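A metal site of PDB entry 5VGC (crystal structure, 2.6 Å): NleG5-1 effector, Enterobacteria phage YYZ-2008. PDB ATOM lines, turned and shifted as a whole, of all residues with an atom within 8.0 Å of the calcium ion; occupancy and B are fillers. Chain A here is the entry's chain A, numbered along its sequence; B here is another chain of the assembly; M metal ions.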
ATOM      1  N   ARG A  99      13.682  16.004  -9.168  1.00  0.00           N
ATOM      2  CA  ARG A  99      14.060  16.071 -10.582  1.00  0.00           C
ATOM      3  C   ARG A  99      13.564  17.376 -11.231  1.00  0.00           C
ATOM      4  O   ARG A  99      14.299  17.979 -12.028  1.00  0.00           O
ATOM      5  CB  ARG A  99      13.522  14.853 -11.338  1.00  0.00           C
ATOM      6  CG  ARG A  99      14.162  14.627 -12.697  1.00  0.00           C
ATOM      7  CD  ARG A  99      15.536  14.008 -12.556  1.00  0.00           C
ATOM      8  NE  ARG A  99      16.134  13.809 -13.865  1.00  0.00           N
ATOM      9  CZ  ARG A  99      16.734  14.762 -14.582  1.00  0.00           C
ATOM     10  NH1 ARG A  99      16.848  16.009 -14.150  1.00  0.00           N
ATOM     11  NH2 ARG A  99      17.251  14.446 -15.775  1.00  0.00           N
ATOM     12  N   GLU A 100      12.339  17.797 -10.892  1.00  0.00           N
ATOM     13  CA  GLU A 100      11.830  19.090 -11.363  1.00  0.00           C
ATOM     14  C   GLU A 100      12.718  20.217 -10.877  1.00  0.00           C
ATOM     15  O   GLU A 100      13.020  21.139 -11.651  1.00  0.00           O
ATOM     16  CB  GLU A 100      10.387  19.335 -10.924  1.00  0.00           C
ATOM     17  CG  GLU A 100       9.346  18.457 -11.611  1.00  0.00           C
ATOM     18  CD  GLU A 100       9.063  18.831 -13.048  1.00  0.00           C
ATOM     19  OE1 GLU A 100       9.661  19.817 -13.564  1.00  0.00           O
ATOM     20  OE2 GLU A 100       8.240  18.126 -13.656  1.00  0.00           O
ATOM     21  N   ILE A 101      13.155  20.159  -9.618  1.00  0.00           N
ATOM     22  CA  ILE A 101      14.148  21.168  -9.177  1.00  0.00           C
ATOM     23  C   ILE A 101      15.397  21.099 -10.046  1.00  0.00           C
ATOM     24  O   ILE A 101      15.857  22.123 -10.535  1.00  0.00           O
ATOM     25  CB  ILE A 101      14.544  21.018  -7.687  1.00  0.00           C
ATOM     26  CG1 ILE A 101      13.348  21.341  -6.804  1.00  0.00           C
ATOM     27  CG2 ILE A 101      15.723  21.940  -7.342  1.00  0.00           C
ATOM     28  CD1 ILE A 101      13.483  20.842  -5.385  1.00  0.00           C
ATOM     29  N   GLU A 102      15.950  19.900 -10.234  1.00  0.00           N
ATOM     30  CA  GLU A 102      17.177  19.742 -11.049  1.00  0.00           C
ATOM     31  C   GLU A 102      17.025  20.316 -12.443  1.00  0.00           C
ATOM     32  O   GLU A 102      17.916  21.021 -12.942  1.00  0.00           O
ATOM     33  CB  GLU A 102      17.601  18.258 -11.128  1.00  0.00           C
ATOM     34  CG  GLU A 102      18.165  17.687  -9.807  1.00  0.00           C
ATOM     35  CD  GLU A 102      18.486  16.201  -9.861  1.00  0.00           C
ATOM     36  OE1 GLU A 102      19.007  15.688  -8.841  1.00  0.00           O
ATOM     37  OE2 GLU A 102      18.216  15.542 -10.898  1.00  0.00           O
ATOM     38  N   MET A 103      15.885  20.039 -13.073  1.00  0.00           N
ATOM     39  CA  MET A 103      15.618  20.441 -14.457  1.00  0.00           C
ATOM     40  C   MET A 103      15.420  21.943 -14.698  1.00  0.00           C
ATOM     41  O   MET A 103      15.295  22.362 -15.835  1.00  0.00           O
ATOM     42  CB  MET A 103      14.423  19.672 -15.014  1.00  0.00           C
ATOM     43  CG  MET A 103      14.753  18.233 -15.346  1.00  0.00           C
ATOM     44  SD  MET A 103      13.406  17.465 -16.252  1.00  0.00           S
ATOM     45  CE  MET A 103      12.389  16.761 -14.949  1.00  0.00           C
ATOM     46  N   LEU A 104      15.388  22.751 -13.649  1.00  0.00           N
ATOM     47  CA  LEU A 104      15.439  24.210 -13.818  1.00  0.00           C
ATOM     48  C   LEU A 104      16.726  24.575 -14.548  1.00  0.00           C
ATOM     49  O   LEU A 104      17.766  23.957 -14.307  1.00  0.00           O
ATOM     50  CB  LEU A 104      15.364  24.955 -12.474  1.00  0.00           C
ATOM     51  CG  LEU A 104      14.035  24.928 -11.726  1.00  0.00           C
ATOM     52  CD1 LEU A 104      14.217  25.269 -10.248  1.00  0.00           C
ATOM     53  CD2 LEU A 104      13.034  25.877 -12.358  1.00  0.00           C
ATOM     54  N   GLU A 105      16.650  25.579 -15.409  1.00  0.00           N
ATOM     55  CA  GLU A 105      17.740  26.013 -16.266  1.00  0.00           C
ATOM     56  C   GLU A 105      18.218  27.409 -15.910  1.00  0.00           C
ATOM     57  O   GLU A 105      17.532  28.170 -15.173  1.00  0.00           O
ATOM     58  CB  GLU A 105      17.273  25.984 -17.731  1.00  0.00           C
ATOM     59  CG  GLU A 105      16.680  24.630 -18.150  1.00  0.00           C
ATOM     60  CD  GLU A 105      16.328  24.539 -19.630  1.00  0.00           C
ATOM     61  OE1 GLU A 105      15.867  25.542 -20.235  1.00  0.00           O
ATOM     62  OE2 GLU A 105      16.509  23.439 -20.207  1.00  0.00           O
ATOM     63  N   ASN A 106      19.402  27.761 -16.420  1.00  0.00           N
ATOM     64  CA  ASN A 106      19.984  29.076 -16.189  1.00  0.00           C
ATOM     65  C   ASN A 106      18.937  30.166 -16.457  1.00  0.00           C
ATOM     66  O   ASN A 106      18.217  30.121 -17.448  1.00  0.00           O
ATOM     67  CB  ASN A 106      21.245  29.284 -17.043  1.00  0.00           C
ATOM     68  CG  ASN A 106      22.348  28.267 -16.731  1.00  0.00           C
ATOM     69  OD1 ASN A 106      22.546  27.872 -15.560  1.00  0.00           O
ATOM     70  ND2 ASN A 106      23.064  27.842 -17.766  1.00  0.00           N
ATOM     71  N   ASP A 108      16.044  30.552 -15.112  1.00  0.00           N
ATOM     72  CA  ASP A 108      14.610  30.188 -14.960  1.00  0.00           C
ATOM     73  C   ASP A 108      13.980  30.794 -13.695  1.00  0.00           C
ATOM     74  O   ASP A 108      12.803  31.181 -13.721  1.00  0.00           O
ATOM     75  CB  ASP A 108      14.396  28.664 -14.925  1.00  0.00           C
ATOM     76  CG  ASP A 108      14.009  28.064 -16.285  1.00  0.00           C
ATOM     77  OD1 ASP A 108      13.568  28.788 -17.199  1.00  0.00           O
ATOM     78  OD2 ASP A 108      14.122  26.807 -16.434  1.00  0.00           O
ATOM     79  N   ARG B  99      20.707  31.282  -7.991  1.00  0.00           N
ATOM     80  CA  ARG B  99      21.603  30.765  -9.017  1.00  0.00           C
ATOM     81  C   ARG B  99      22.134  29.369  -8.649  1.00  0.00           C
ATOM     82  O   ARG B  99      22.216  28.507  -9.502  1.00  0.00           O
ATOM     83  CB  ARG B  99      22.745  31.737  -9.289  1.00  0.00           C
ATOM     84  CG  ARG B  99      23.468  31.496 -10.591  1.00  0.00           C
ATOM     85  CD  ARG B  99      22.676  31.945 -11.807  1.00  0.00           C
ATOM     86  NE  ARG B  99      23.463  31.682 -13.011  1.00  0.00           N
ATOM     87  CZ  ARG B  99      23.551  30.511 -13.624  1.00  0.00           C
ATOM     88  NH1 ARG B  99      22.900  29.428 -13.181  1.00  0.00           N
ATOM     89  NH2 ARG B  99      24.312  30.410 -14.713  1.00  0.00           N
ATOM     90  N   GLU B 100      22.494  29.174  -7.380  1.00  0.00           N
ATOM     91  CA  GLU B 100      22.902  27.848  -6.882  1.00  0.00           C
ATOM     92  C   GLU B 100      21.781  26.859  -7.080  1.00  0.00           C
ATOM     93  O   GLU B 100      22.038  25.728  -7.499  1.00  0.00           O
ATOM     94  CB  GLU B 100      23.321  27.872  -5.412  1.00  0.00           C
ATOM     95  CG  GLU B 100      24.641  28.567  -5.134  1.00  0.00           C
ATOM     96  CD  GLU B 100      25.854  27.758  -5.536  1.00  0.00           C
ATOM     97  OE1 GLU B 100      25.713  26.607  -6.009  1.00  0.00           O
ATOM     98  OE2 GLU B 100      26.989  28.274  -5.354  1.00  0.00           O
ATOM     99  N   ILE B 101      20.534  27.262  -6.795  1.00  0.00           N
ATOM    100  CA  ILE B 101      19.423  26.347  -7.120  1.00  0.00           C
ATOM    101  C   ILE B 101      19.422  26.018  -8.624  1.00  0.00           C
ATOM    102  O   ILE B 101      19.380  24.831  -9.001  1.00  0.00           O
ATOM    103  CB  ILE B 101      18.038  26.891  -6.717  1.00  0.00           C
ATOM    104  CG1 ILE B 101      17.933  26.995  -5.208  1.00  0.00           C
ATOM    105  CG2 ILE B 101      16.931  25.968  -7.243  1.00  0.00           C
ATOM    106  CD1 ILE B 101      16.822  27.907  -4.739  1.00  0.00           C
ATOM    107  N   GLU B 102      19.474  27.065  -9.457  1.00  0.00           N
ATOM    108  CA  GLU B 102      19.475  26.846 -10.926  1.00  0.00           C
ATOM    109  C   GLU B 102      20.599  25.884 -11.392  1.00  0.00           C
ATOM    110  O   GLU B 102      20.364  24.979 -12.199  1.00  0.00           O
ATOM    111  CB  GLU B 102      19.587  28.183 -11.679  1.00  0.00           C
ATOM    112  CG  GLU B 102      18.354  29.085 -11.596  1.00  0.00           C
ATOM    113  CD  GLU B 102      18.501  30.411 -12.315  1.00  0.00           C
ATOM    114  OE1 GLU B 102      17.504  31.186 -12.327  1.00  0.00           O
ATOM    115  OE2 GLU B 102      19.590  30.677 -12.891  1.00  0.00           O
ATOM    116  N   MET B 103      21.796  26.091 -10.851  1.00  0.00           N
ATOM    117  CA  MET B 103      22.989  25.373 -11.272  1.00  0.00           C
ATOM    118  C   MET B 103      23.032  23.891 -10.871  1.00  0.00           C
ATOM    119  O   MET B 103      23.978  23.192 -11.277  1.00  0.00           O
ATOM    120  CB  MET B 103      24.248  26.039 -10.718  1.00  0.00           C
ATOM    121  CG  MET B 103      24.668  27.308 -11.410  1.00  0.00           C
ATOM    122  SD  MET B 103      26.223  27.886 -10.704  1.00  0.00           S
ATOM    123  CE  MET B 103      26.353  29.533 -11.385  1.00  0.00           C
ATOM    124  N   LEU B 104      22.052  23.408 -10.095  1.00  0.00           N
ATOM    125  CA  LEU B 104      21.928  21.971  -9.867  1.00  0.00           C
ATOM    126  C   LEU B 104      21.767  21.272 -11.216  1.00  0.00           C
ATOM    127  O   LEU B 104      21.113  21.799 -12.136  1.00  0.00           O
ATOM    128  CB  LEU B 104      20.743  21.638  -8.962  1.00  0.00           C
ATOM    129  CG  LEU B 104      20.862  22.013  -7.474  1.00  0.00           C
ATOM    130  CD1 LEU B 104      19.502  22.054  -6.789  1.00  0.00           C
ATOM    131  CD2 LEU B 104      21.810  21.067  -6.737  1.00  0.00           C
ATOM    132  N   GLU B 105      22.393  20.092 -11.306  1.00  0.00           N
ATOM    133  CA  GLU B 105      22.381  19.275 -12.513  1.00  0.00           C
ATOM    134  C   GLU B 105      21.657  17.964 -12.260  1.00  0.00           C
ATOM    135  O   GLU B 105      21.460  17.532 -11.099  1.00  0.00           O
ATOM    136  CB  GLU B 105      23.817  18.998 -12.997  1.00  0.00           C
ATOM    137  CG  GLU B 105      24.661  20.274 -13.143  1.00  0.00           C
ATOM    138  CD  GLU B 105      26.078  20.031 -13.630  1.00  0.00           C
ATOM    139  OE1 GLU B 105      26.276  19.165 -14.514  1.00  0.00           O
ATOM    140  OE2 GLU B 105      26.994  20.723 -13.121  1.00  0.00           O
ATOM    141  N   ASN B 106      21.260  17.327 -13.370  1.00  0.00           N
ATOM    142  CA  ASN B 106      20.669  15.991 -13.323  1.00  0.00           C
ATOM    143  C   ASN B 106      21.450  15.078 -12.349  1.00  0.00           C
ATOM    144  O   ASN B 106      22.691  15.026 -12.380  1.00  0.00           O
ATOM    145  CB  ASN B 106      20.521  15.353 -14.720  1.00  0.00           C
ATOM    146  CG  ASN B 106      21.594  15.784 -15.717  1.00  0.00           C
ATOM    147  OD1 ASN B 106      21.427  16.786 -16.422  1.00  0.00           O
ATOM    148  ND2 ASN B 106      22.678  15.028 -15.790  1.00  0.00           N
ATOM    149  N   ASP B 108      22.142  15.526  -9.243  1.00  0.00           N
ATOM    150  CA  ASP B 108      22.925  16.155  -8.160  1.00  0.00           C
ATOM    151  C   ASP B 108      22.328  15.944  -6.761  1.00  0.00           C
ATOM    152  O   ASP B 108      23.060  15.796  -5.788  1.00  0.00           O
ATOM    153  CB  ASP B 108      23.144  17.671  -8.394  1.00  0.00           C
ATOM    154  CG  ASP B 108      24.492  18.011  -9.048  1.00  0.00           C
ATOM    155  OD1 ASP B 108      25.422  17.172  -9.054  1.00  0.00           O
ATOM    156  OD2 ASP B 108      24.617  19.150  -9.554  1.00  0.00           O
HETATM  157 CA    CA M   1      19.343  22.824 -13.144  1.00  0.00          CA
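Along chain A the residues within 4 Å of the calcium ion span positions 102 to 104.
OE1 of Glu 102 of chain B is in hydrogen-bond range of N of Asp 108 of chain A (3.2 Å).
The guanidinium group (NH1) of Arg 99 of chain A lies within salt-bridge range of the side-chain carboxylate (OE2) of Glu 102 of chain A, 3.6 Å away.
The backbone NH (N) of Asp 108 of chain B sits at hydrogen-bond distance from the side-chain carboxylate (OE1) of Glu 102 of chain A (3.2 Å).
NH1 of Arg 99 of chain B is in salt-bridge range of OE2 of Glu 102 of chain B (3.5 Å).
The calcium ion is bound by O of Leu 104 of chain A (2.3 Å), O of Leu 104 of chain B (2.3 Å), O of Glu 102 of chain A (2.3 Å) and O of Glu 102 of chain B (2.6 Å).
The calcium ion has four donor atoms within binding distance.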
